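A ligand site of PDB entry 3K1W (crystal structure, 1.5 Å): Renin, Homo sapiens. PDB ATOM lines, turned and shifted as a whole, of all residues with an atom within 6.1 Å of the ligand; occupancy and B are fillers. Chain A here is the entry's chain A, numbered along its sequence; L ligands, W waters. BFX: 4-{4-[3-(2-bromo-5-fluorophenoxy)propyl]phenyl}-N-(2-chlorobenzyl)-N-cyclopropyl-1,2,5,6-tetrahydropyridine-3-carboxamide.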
ATOM      1  N   THR A  18       2.195   0.283  29.911  1.00  0.00           N
ATOM      2  CA  THR A  18       2.298   1.751  29.956  1.00  0.00           C
ATOM      3  C   THR A  18       1.526   2.468  28.877  1.00  0.00           C
ATOM      4  O   THR A  18       1.326   3.681  28.984  1.00  0.00           O
ATOM      5  CB  THR A  18       3.792   2.227  29.879  1.00  0.00           C
ATOM      6  OG1 THR A  18       4.376   1.741  28.641  1.00  0.00           O
ATOM      7  CG2 THR A  18       4.638   1.626  31.010  1.00  0.00           C
ATOM      8  N   GLN A  19       1.154   1.739  27.840  1.00  0.00           N
ATOM      9  CA  GLN A  19       0.386   2.349  26.731  1.00  0.00           C
ATOM     10  C   GLN A  19      -0.748   1.427  26.360  1.00  0.00           C
ATOM     11  O   GLN A  19      -0.521   0.243  26.084  1.00  0.00           O
ATOM     12  CB  GLN A  19       1.282   2.563  25.507  1.00  0.00           C
ATOM     13  CG  GLN A  19       2.595   3.328  25.802  1.00  0.00           C
ATOM     14  CD  GLN A  19       3.441   3.514  24.558  1.00  0.00           C
ATOM     15  OE1 GLN A  19       2.983   3.241  23.422  1.00  0.00           O
ATOM     16  NE2 GLN A  19       4.673   3.981  24.746  1.00  0.00           N
ATOM     17  N   VAL A  36      -4.602   6.337  21.908  1.00  0.00           N
ATOM     18  CA  VAL A  36      -4.938   6.268  23.344  1.00  0.00           C
ATOM     19  C   VAL A  36      -6.215   7.038  23.580  1.00  0.00           C
ATOM     20  O   VAL A  36      -6.353   8.172  23.075  1.00  0.00           O
ATOM     21  CB  VAL A  36      -3.816   6.892  24.224  1.00  0.00           C
ATOM     22  CG1 VAL A  36      -4.252   6.999  25.717  1.00  0.00           C
ATOM     23  CG2 VAL A  36      -2.574   6.039  24.123  1.00  0.00           C
ATOM     24  N   ASP A  38      -8.051   9.039  26.143  1.00  0.00           N
ATOM     25  CA  ASP A  38      -7.368   9.770  27.244  1.00  0.00           C
ATOM     26  C   ASP A  38      -8.304  10.700  27.997  1.00  0.00           C
ATOM     27  O   ASP A  38      -8.673  11.738  27.468  1.00  0.00           O
ATOM     28  CB  ASP A  38      -6.251  10.571  26.619  1.00  0.00           C
ATOM     29  CG  ASP A  38      -5.489  11.441  27.599  1.00  0.00           C
ATOM     30  OD1 ASP A  38      -5.399  11.080  28.805  1.00  0.00           O
ATOM     31  OD2 ASP A  38      -4.883  12.460  27.167  1.00  0.00           O
ATOM     32  N   THR A  39      -8.697  10.326  29.217  1.00  0.00           N
ATOM     33  CA  THR A  39      -9.601  11.210  30.003  1.00  0.00           C
ATOM     34  C   THR A  39      -8.911  12.462  30.533  1.00  0.00           C
ATOM     35  O   THR A  39      -9.571  13.394  31.030  1.00  0.00           O
ATOM     36  CB  THR A  39     -10.250  10.426  31.169  1.00  0.00           C
ATOM     37  OG1 THR A  39      -9.206   9.747  31.896  1.00  0.00           O
ATOM     38  CG2 THR A  39     -11.188   9.330  30.641  1.00  0.00           C
ATOM     39  N   GLY A  40      -7.603  12.515  30.420  1.00  0.00           N
ATOM     40  CA  GLY A  40      -6.837  13.660  30.863  1.00  0.00           C
ATOM     41  C   GLY A  40      -6.597  14.703  29.792  1.00  0.00           C
ATOM     42  O   GLY A  40      -5.793  15.612  29.972  1.00  0.00           O
ATOM     43  N   SER A  41      -7.282  14.579  28.655  1.00  0.00           N
ATOM     44  CA  SER A  41      -7.255  15.648  27.658  1.00  0.00           C
ATOM     45  C   SER A  41      -8.538  15.637  26.844  1.00  0.00           C
ATOM     46  O   SER A  41      -9.351  14.707  26.968  1.00  0.00           O
ATOM     47  CB  SER A  41      -6.041  15.543  26.772  1.00  0.00           C
ATOM     48  OG  SER A  41      -6.130  14.421  25.941  1.00  0.00           O
ATOM     49  N   TRP A  45      -6.031  14.257  18.328  1.00  0.00           N
ATOM     50  CA  TRP A  45      -4.803  14.572  17.596  1.00  0.00           C
ATOM     51  C   TRP A  45      -4.360  13.348  16.800  1.00  0.00           C
ATOM     52  O   TRP A  45      -4.307  12.227  17.368  1.00  0.00           O
ATOM     53  CB  TRP A  45      -3.654  14.875  18.561  1.00  0.00           C
ATOM     54  CG  TRP A  45      -3.707  16.148  19.408  1.00  0.00           C
ATOM     55  CD1 TRP A  45      -4.034  16.235  20.729  1.00  0.00           C
ATOM     56  CD2 TRP A  45      -3.317  17.462  18.994  1.00  0.00           C
ATOM     57  NE1 TRP A  45      -3.913  17.540  21.157  1.00  0.00           N
ATOM     58  CE2 TRP A  45      -3.472  18.310  20.114  1.00  0.00           C
ATOM     59  CE3 TRP A  45      -2.874  18.026  17.788  1.00  0.00           C
ATOM     60  CZ2 TRP A  45      -3.202  19.685  20.062  1.00  0.00           C
ATOM     61  CZ3 TRP A  45      -2.603  19.400  17.736  1.00  0.00           C
ATOM     62  CH2 TRP A  45      -2.754  20.204  18.887  1.00  0.00           C
ATOM     63  N   VAL A  46      -3.994  13.547  15.528  1.00  0.00           N
ATOM     64  CA  VAL A  46      -3.294  12.526  14.730  1.00  0.00           C
ATOM     65  C   VAL A  46      -2.163  13.237  13.980  1.00  0.00           C
ATOM     66  O   VAL A  46      -2.263  14.470  13.798  1.00  0.00           O
ATOM     67  CB  VAL A  46      -4.219  11.799  13.713  1.00  0.00           C
ATOM     68  CG1 VAL A  46      -5.184  10.829  14.429  1.00  0.00           C
ATOM     69  CG2 VAL A  46      -4.991  12.813  12.866  1.00  0.00           C
ATOM     70  N   PRO A  47      -1.078  12.543  13.605  1.00  0.00           N
ATOM     71  CA  PRO A  47      -0.005  13.206  12.857  1.00  0.00           C
ATOM     72  C   PRO A  47      -0.513  13.609  11.467  1.00  0.00           C
ATOM     73  O   PRO A  47      -1.363  12.910  10.884  1.00  0.00           O
ATOM     74  CB  PRO A  47       1.079  12.127  12.737  1.00  0.00           C
ATOM     75  CG  PRO A  47       0.749  11.132  13.776  1.00  0.00           C
ATOM     76  CD  PRO A  47      -0.782  11.127  13.848  1.00  0.00           C
ATOM     77  N   ALA A  57       9.141  11.866  15.754  1.00  0.00           N
ATOM     78  CA  ALA A  57       7.813  11.641  16.359  1.00  0.00           C
ATOM     79  C   ALA A  57       6.712  11.418  15.317  1.00  0.00           C
ATOM     80  O   ALA A  57       5.641  10.899  15.647  1.00  0.00           O
ATOM     81  CB  ALA A  57       7.449  12.786  17.252  1.00  0.00           C
ATOM     82  N   HIS A  61       5.084   6.906  12.610  1.00  0.00           N
ATOM     83  CA  HIS A  61       3.649   6.769  12.876  1.00  0.00           C
ATOM     84  C   HIS A  61       2.846   6.923  11.576  1.00  0.00           C
ATOM     85  O   HIS A  61       3.386   7.378  10.555  1.00  0.00           O
ATOM     86  CB  HIS A  61       3.206   7.791  13.888  1.00  0.00           C
ATOM     87  CG  HIS A  61       3.763   7.547  15.262  1.00  0.00           C
ATOM     88  ND1 HIS A  61       4.507   8.488  15.942  1.00  0.00           N
ATOM     89  CD2 HIS A  61       3.705   6.450  16.050  1.00  0.00           C
ATOM     90  CE1 HIS A  61       4.860   7.974  17.114  1.00  0.00           C
ATOM     91  NE2 HIS A  61       4.403   6.743  17.198  1.00  0.00           N
ATOM     92  N   LEU A  81      -0.003  23.119  21.826  1.00  0.00           N
ATOM     93  CA  LEU A  81       0.127  22.633  23.192  1.00  0.00           C
ATOM     94  C   LEU A  81       1.567  22.788  23.632  1.00  0.00           C
ATOM     95  O   LEU A  81       2.485  22.210  23.037  1.00  0.00           O
ATOM     96  CB  LEU A  81      -0.297  21.175  23.290  1.00  0.00           C
ATOM     97  CG  LEU A  81      -0.188  20.521  24.658  1.00  0.00           C
ATOM     98  CD1 LEU A  81      -1.194  21.115  25.646  1.00  0.00           C
ATOM     99  CD2 LEU A  81      -0.382  19.024  24.543  1.00  0.00           C
ATOM    100  N   TYR A  83       3.765  21.526  25.636  1.00  0.00           N
ATOM    101  CA  TYR A  83       4.064  20.312  26.370  1.00  0.00           C
ATOM    102  C   TYR A  83       5.423  20.395  27.091  1.00  0.00           C
ATOM    103  O   TYR A  83       6.259  21.212  26.733  1.00  0.00           O
ATOM    104  CB  TYR A  83       4.010  19.112  25.410  1.00  0.00           C
ATOM    105  CG  TYR A  83       4.143  17.787  26.102  1.00  0.00           C
ATOM    106  CD1 TYR A  83       5.346  17.093  26.121  1.00  0.00           C
ATOM    107  CD2 TYR A  83       3.048  17.237  26.777  1.00  0.00           C
ATOM    108  CE1 TYR A  83       5.470  15.876  26.774  1.00  0.00           C
ATOM    109  CE2 TYR A  83       3.158  16.015  27.438  1.00  0.00           C
ATOM    110  CZ  TYR A  83       4.362  15.350  27.439  1.00  0.00           C
ATOM    111  OH  TYR A  83       4.473  14.157  28.107  1.00  0.00           O
ATOM    112  N   VAL A  88       3.934  20.974  20.813  1.00  0.00           N
ATOM    113  CA  VAL A  88       3.134  20.221  19.833  1.00  0.00           C
ATOM    114  C   VAL A  88       2.217  21.225  19.114  1.00  0.00           C
ATOM    115  O   VAL A  88       1.400  21.894  19.747  1.00  0.00           O
ATOM    116  CB  VAL A  88       2.277  19.095  20.528  1.00  0.00           C
ATOM    117  CG1 VAL A  88       1.373  18.349  19.501  1.00  0.00           C
ATOM    118  CG2 VAL A  88       3.194  18.097  21.263  1.00  0.00           C
ATOM    119  N   VAL A 111      -1.206  17.147  13.640  1.00  0.00           N
ATOM    120  CA  VAL A 111       0.088  17.590  14.134  1.00  0.00           C
ATOM    121  C   VAL A 111       1.135  17.751  13.015  1.00  0.00           C
ATOM    122  O   VAL A 111       1.350  16.828  12.253  1.00  0.00           O
ATOM    123  CB  VAL A 111       0.608  16.587  15.175  1.00  0.00           C
ATOM    124  CG1 VAL A 111       2.000  17.009  15.697  1.00  0.00           C
ATOM    125  CG2 VAL A 111      -0.382  16.485  16.358  1.00  0.00           C
ATOM    126  N   MET A 114       6.195  18.051  16.686  1.00  0.00           N
ATOM    127  CA  MET A 114       6.116  17.687  18.106  1.00  0.00           C
ATOM    128  C   MET A 114       7.465  17.140  18.459  1.00  0.00           C
ATOM    129  O   MET A 114       8.151  16.590  17.587  1.00  0.00           O
ATOM    130  CB  MET A 114       4.991  16.656  18.363  1.00  0.00           C
ATOM    131  CG  MET A 114       5.013  15.456  17.466  1.00  0.00           C
ATOM    132  SD  MET A 114       3.713  14.274  17.962  1.00  0.00           S
ATOM    133  CE  MET A 114       3.517  13.392  16.415  1.00  0.00           C
ATOM    134  N   PRO A 118       8.544  12.657  24.496  1.00  0.00           N
ATOM    135  CA  PRO A 118       8.447  11.199  24.529  1.00  0.00           C
ATOM    136  C   PRO A 118       7.771  10.559  23.308  1.00  0.00           C
ATOM    137  O   PRO A 118       7.737   9.322  23.210  1.00  0.00           O
ATOM    138  CB  PRO A 118       7.564  10.967  25.754  1.00  0.00           C
ATOM    139  CG  PRO A 118       6.656  12.145  25.814  1.00  0.00           C
ATOM    140  CD  PRO A 118       7.407  13.302  25.168  1.00  0.00           C
ATOM    141  N   PHE A 119       7.284  11.388  22.384  1.00  0.00           N
ATOM    142  CA  PHE A 119       6.362  10.898  21.350  1.00  0.00           C
ATOM    143  C   PHE A 119       6.903   9.873  20.364  1.00  0.00           C
ATOM    144  O   PHE A 119       6.126   9.082  19.833  1.00  0.00           O
ATOM    145  CB  PHE A 119       5.656  12.087  20.685  1.00  0.00           C
ATOM    146  CG  PHE A 119       5.047  13.017  21.679  1.00  0.00           C
ATOM    147  CD1 PHE A 119       4.044  12.568  22.551  1.00  0.00           C
ATOM    148  CD2 PHE A 119       5.501  14.321  21.828  1.00  0.00           C
ATOM    149  CE1 PHE A 119       3.475  13.424  23.501  1.00  0.00           C
ATOM    150  CE2 PHE A 119       4.954  15.182  22.783  1.00  0.00           C
ATOM    151  CZ  PHE A 119       3.922  14.732  23.629  1.00  0.00           C
ATOM    152  N   MET A 120       8.218   9.855  20.137  1.00  0.00           N
ATOM    153  CA  MET A 120       8.792   8.842  19.278  1.00  0.00           C
ATOM    154  C   MET A 120       8.676   7.435  19.883  1.00  0.00           C
ATOM    155  O   MET A 120       8.759   6.440  19.164  1.00  0.00           O
ATOM    156  CB  MET A 120      10.259   9.163  18.915  1.00  0.00           C
ATOM    157  CG  MET A 120      11.275   8.663  19.917  1.00  0.00           C
ATOM    158  SD  MET A 120      12.971   9.153  19.448  1.00  0.00           S
ATOM    159  CE  MET A 120      13.237   8.080  18.041  1.00  0.00           C
ATOM    160  N   LEU A 121       8.463   7.361  21.204  1.00  0.00           N
ATOM    161  CA  LEU A 121       8.448   6.071  21.911  1.00  0.00           C
ATOM    162  C   LEU A 121       7.022   5.562  22.041  1.00  0.00           C
ATOM    163  O   LEU A 121       6.786   4.483  22.620  1.00  0.00           O
ATOM    164  CB  LEU A 121       9.106   6.194  23.281  1.00  0.00           C
ATOM    165  CG  LEU A 121      10.560   6.729  23.216  1.00  0.00           C
ATOM    166  CD1 LEU A 121      11.079   7.124  24.595  1.00  0.00           C
ATOM    167  CD2 LEU A 121      11.499   5.758  22.543  1.00  0.00           C
ATOM    168  N   ALA A 122       6.062   6.330  21.515  1.00  0.00           N
ATOM    169  CA  ALA A 122       4.684   5.867  21.487  1.00  0.00           C
ATOM    170  C   ALA A 122       4.510   4.776  20.436  1.00  0.00           C
ATOM    171  O   ALA A 122       4.950   4.961  19.277  1.00  0.00           O
ATOM    172  CB  ALA A 122       3.741   7.020  21.212  1.00  0.00           C
ATOM    173  N   PHE A 124       1.464   3.928  19.649  1.00  0.00           N
ATOM    174  CA  PHE A 124       0.217   4.404  19.056  1.00  0.00           C
ATOM    175  C   PHE A 124       0.496   5.650  18.206  1.00  0.00           C
ATOM    176  O   PHE A 124       1.553   6.283  18.323  1.00  0.00           O
ATOM    177  CB  PHE A 124      -0.760   4.732  20.176  1.00  0.00           C
ATOM    178  CG  PHE A 124      -0.222   5.691  21.211  1.00  0.00           C
ATOM    179  CD1 PHE A 124       0.495   5.223  22.335  1.00  0.00           C
ATOM    180  CD2 PHE A 124      -0.416   7.074  21.058  1.00  0.00           C
ATOM    181  CE1 PHE A 124       0.969   6.139  23.293  1.00  0.00           C
ATOM    182  CE2 PHE A 124       0.080   7.976  21.997  1.00  0.00           C
ATOM    183  CZ  PHE A 124       0.775   7.496  23.101  1.00  0.00           C
ATOM    184  N   ASP A 125      -0.453   5.981  17.326  1.00  0.00           N
ATOM    185  CA  ASP A 125      -0.312   7.076  16.364  1.00  0.00           C
ATOM    186  C   ASP A 125      -0.942   8.379  16.799  1.00  0.00           C
ATOM    187  O   ASP A 125      -0.595   9.433  16.281  1.00  0.00           O
ATOM    188  CB  ASP A 125      -1.010   6.692  15.042  1.00  0.00           C
ATOM    189  CG  ASP A 125      -0.520   5.389  14.505  1.00  0.00           C
ATOM    190  OD1 ASP A 125       0.680   5.290  14.198  1.00  0.00           O
ATOM    191  OD2 ASP A 125      -1.273   4.389  14.388  1.00  0.00           O
ATOM    192  N   GLY A 126      -1.895   8.318  17.726  1.00  0.00           N
ATOM    193  CA  GLY A 126      -2.660   9.515  18.030  1.00  0.00           C
ATOM    194  C   GLY A 126      -3.320   9.457  19.409  1.00  0.00           C
ATOM    195  O   GLY A 126      -3.137   8.504  20.158  1.00  0.00           O
ATOM    196  N   VAL A 127      -4.084  10.498  19.710  1.00  0.00           N
ATOM    197  CA  VAL A 127      -4.748  10.626  21.005  1.00  0.00           C
ATOM    198  C   VAL A 127      -6.213  11.017  20.784  1.00  0.00           C
ATOM    199  O   VAL A 127      -6.489  11.895  19.960  1.00  0.00           O
ATOM    200  CB  VAL A 127      -4.060  11.696  21.880  1.00  0.00           C
ATOM    201  CG1 VAL A 127      -4.699  11.786  23.235  1.00  0.00           C
ATOM    202  CG2 VAL A 127      -2.532  11.413  22.030  1.00  0.00           C
ATOM    203  N   LEU A 224      -7.050  13.184  39.699  1.00  0.00           N
ATOM    204  CA  LEU A 224      -7.433  13.180  38.287  1.00  0.00           C
ATOM    205  C   LEU A 224      -7.427  11.710  37.893  1.00  0.00           C
ATOM    206  O   LEU A 224      -6.480  11.016  38.206  1.00  0.00           O
ATOM    207  CB  LEU A 224      -6.383  13.944  37.484  1.00  0.00           C
ATOM    208  CG  LEU A 224      -6.530  13.913  35.961  1.00  0.00           C
ATOM    209  CD1 LEU A 224      -7.797  14.639  35.475  1.00  0.00           C
ATOM    210  CD2 LEU A 224      -5.292  14.515  35.302  1.00  0.00           C
ATOM    211  N   ASP A 226      -6.969   9.450  35.053  1.00  0.00           N
ATOM    212  CA  ASP A 226      -6.399   9.753  33.738  1.00  0.00           C
ATOM    213  C   ASP A 226      -6.058   8.471  32.960  1.00  0.00           C
ATOM    214  O   ASP A 226      -4.997   7.863  33.143  1.00  0.00           O
ATOM    215  CB  ASP A 226      -5.163  10.635  33.901  1.00  0.00           C
ATOM    216  CG  ASP A 226      -4.575  11.047  32.573  1.00  0.00           C
ATOM    217  OD1 ASP A 226      -5.063  10.588  31.509  1.00  0.00           O
ATOM    218  OD2 ASP A 226      -3.612  11.853  32.509  1.00  0.00           O
ATOM    219  N   GLY A 228      -5.069   8.025  30.047  1.00  0.00           N
ATOM    220  CA  GLY A 228      -3.922   8.171  29.148  1.00  0.00           C
ATOM    221  C   GLY A 228      -2.578   8.213  29.855  1.00  0.00           C
ATOM    222  O   GLY A 228      -1.546   8.278  29.158  1.00  0.00           O
ATOM    223  N   ALA A 229      -2.568   8.233  31.187  1.00  0.00           N
ATOM    224  CA  ALA A 229      -1.334   8.255  31.971  1.00  0.00           C
ATOM    225  C   ALA A 229      -0.899   6.819  32.267  1.00  0.00           C
ATOM    226  O   ALA A 229      -1.755   5.944  32.517  1.00  0.00           O
ATOM    227  CB  ALA A 229      -1.577   8.984  33.247  1.00  0.00           C
ATOM    228  N   SER A 230       0.416   6.557  32.219  1.00  0.00           N
ATOM    229  CA  SER A 230       0.870   5.189  32.430  1.00  0.00           C
ATOM    230  C   SER A 230       0.796   4.780  33.880  1.00  0.00           C
ATOM    231  O   SER A 230       0.534   3.624  34.209  1.00  0.00           O
ATOM    232  CB  SER A 230       2.320   5.048  31.980  1.00  0.00           C
ATOM    233  OG  SER A 230       2.504   5.429  30.623  1.00  0.00           O
HETATM  234 BR1  BFX L   1      -0.361  12.874  17.168  1.00  0.00          BR
HETATM  235  C2  BFX L   1       0.643  11.880  18.429  1.00  0.00           C
HETATM  236  C3  BFX L   1       0.638  12.361  19.705  1.00  0.00           C
HETATM  237  C4  BFX L   1       1.319  10.737  18.083  1.00  0.00           C
HETATM  238  O5  BFX L   1      -0.038  13.490  19.994  1.00  0.00           O
HETATM  239  C6  BFX L   1       1.364  11.687  20.678  1.00  0.00           C
HETATM  240  C7  BFX L   1       2.037  10.039  19.053  1.00  0.00           C
HETATM  241  C8  BFX L   1       0.251  14.180  21.215  1.00  0.00           C
HETATM  242  C9  BFX L   1       2.047  10.532  20.337  1.00  0.00           C
HETATM  243  C10 BFX L   1      -0.785  15.260  21.397  1.00  0.00           C
HETATM  244  F11 BFX L   1       2.739   9.869  21.280  1.00  0.00           F
HETATM  245  C12 BFX L   1      -0.407  16.080  22.620  1.00  0.00           C
HETATM  246  C13 BFX L   1      -0.702  15.390  23.944  1.00  0.00           C
HETATM  247  C14 BFX L   1       0.331  15.068  24.833  1.00  0.00           C
HETATM  248  C15 BFX L   1      -2.011  15.114  24.307  1.00  0.00           C
HETATM  249  C16 BFX L   1       0.098  14.450  26.063  1.00  0.00           C
HETATM  250  C17 BFX L   1      -2.273  14.491  25.521  1.00  0.00           C
HETATM  251  C18 BFX L   1      -1.239  14.169  26.410  1.00  0.00           C
HETATM  252  C19 BFX L   1      -1.618  13.522  27.721  1.00  0.00           C
HETATM  253  C20 BFX L   1      -1.104  12.377  28.214  1.00  0.00           C
HETATM  254  C21 BFX L   1      -2.637  14.330  28.500  1.00  0.00           C
HETATM  255  C22 BFX L   1       0.103  11.789  27.663  1.00  0.00           C
HETATM  256  C23 BFX L   1      -1.701  11.687  29.429  1.00  0.00           C
HETATM  257  C24 BFX L   1      -2.843  13.814  29.913  1.00  0.00           C
HETATM  258  O25 BFX L   1       1.124  11.889  28.343  1.00  0.00           O
HETATM  259  N26 BFX L   1       0.093  11.175  26.481  1.00  0.00           N
HETATM  260  N27 BFX L   1      -2.889  12.358  29.926  1.00  0.00           N
HETATM  261  C28 BFX L   1      -1.101  11.054  25.614  1.00  0.00           C
HETATM  262  C29 BFX L   1       1.347  10.676  25.893  1.00  0.00           C
HETATM  263  C30 BFX L   1      -2.247  10.229  26.198  1.00  0.00           C
HETATM  264  C31 BFX L   1      -1.327   9.601  25.161  1.00  0.00           C
HETATM  265  C32 BFX L   1       1.780   9.317  26.438  1.00  0.00           C
HETATM  266  C33 BFX L   1       2.906   8.690  25.941  1.00  0.00           C
HETATM  267  C34 BFX L   1       1.068   8.636  27.416  1.00  0.00           C
HETATM  268 CL35 BFX L   1       3.876   9.465  24.681  1.00  0.00          CL
HETATM  269  C36 BFX L   1       3.346   7.445  26.357  1.00  0.00           C
HETATM  270  C37 BFX L   1       1.500   7.376  27.870  1.00  0.00           C
HETATM  271  C38 BFX L   1       2.636   6.786  27.325  1.00  0.00           C
HETATM  272  O   HOH W   1       5.047   6.093  29.692  1.00  0.00           O
HETATM  273  O   HOH W   2       5.788   8.967  28.321  1.00  0.00           O
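O of Thr 18 touches C38 of the ligand (3.8 Å).
CG of Gln 19 touches C38 of the ligand (3.8 Å).
Val 36 touches the ligand (CB to C31, 3.8 Å).
O of Gly 40 touches C24 of the ligand, at 3.5 Å.
Ser 41 touches the ligand (OG to C17, 3.9 Å).
CD1 of Trp 45 touches C10 of the ligand, at 3.5 Å.
C of Val 46 touches BR1 of the ligand (3.7 Å).
N of Pro 47 touches BR1 of the ligand, 3.6 Å away.
His 61 touches the ligand (CE1 to C7, 3.999 Å).
CD2 of Leu 81 touches C12 of the ligand, 3.5 Å away.
CE2 of Tyr 83 touches C16 of the ligand (3.7 Å).
CG2 of Val 111 touches BR1 of the ligand, at 3.7 Å.
CE of Met 114 touches C2 of the ligand, at 3.8 Å.
Phe 119 touches the ligand (CD1 to F11, 3.3 Å).
Ala 122 touches the ligand (CB to F11, 3.0 Å).
Phe 124 touches the ligand (CE2 to F11, 3.3 Å).
Asp 125 touches the ligand.
CG2 of Val 127 touches C31 of the ligand, at 3.8 Å.
Gly 228 touches the ligand (O to C34, 3.2 Å).
N of Ala 229 touches C23 of the ligand, at 3.97 Å.
Ser 230 touches the ligand (OG to C37, 3.5 Å).
Hydrophobic or aromatic side chains that line the ligand: Val 36, Trp 45, Pro 47, His 61, Leu 81, Tyr 83, Val 111, Met 114, Phe 119, Ala 122, Phe 124 and Val 127.
23 residues have an atom within 4 Å of the ligand: Thr 18, Gln 19, Val 36, Asp 38, Gly 40, Ser 41, Trp 45, Val 46, Pro 47, His 61, Leu 81, Tyr 83, Val 111, Met 114, Phe 119, Ala 122, Phe 124, Asp 125, Val 127, Asp 226, Gly 228, Ala 229 and Ser 230.
Along chain A the residues within 4 Å of the ligand span positions 18 to 230.
The nearest printed residue that does not touch the ligand is Pro 118 (4.02 Å).
The side-chain carboxylate (OD1) of Asp 226 lies within hydrogen-bond range of the backbone NH (N) of Gly 228.
N of Ala 229 sits at hydrogen-bond distance from OD1 of Asp 226, 3.4 Å away.
The backbone carbonyl oxygen (O) of Ala 122 sits at hydrogen-bond distance from a ring nitrogen (NE2) of His 61, 2.8 Å away.
The side-chain carboxylate (OD2) of Asp 38 is in hydrogen-bond range of the side-chain hydroxyl (OG) of Ser 41.
O of Val 127 lies within hydrogen-bond range of N of Trp 45 (2.9 Å).
The side-chain hydroxyl (OG) of Ser 230 lies within hydrogen-bond range of the backbone carbonyl oxygen (O) of Thr 18 (2.7 Å).
N of Val 36 lies within hydrogen-bond range of O of Gly 126.
ND1 of His 61 sits at hydrogen-bond distance from O of Ala 57 (2.7 Å).
The side-chain carboxylate of Asp 226 lies within salt-bridge range of a nitrogen (N27) of the ligand (2.7 Å).
The side-chain carboxylate (OD1) of Asp 38 lies within salt-bridge range of a nitrogen (N27) of the ligand (3.0 Å).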
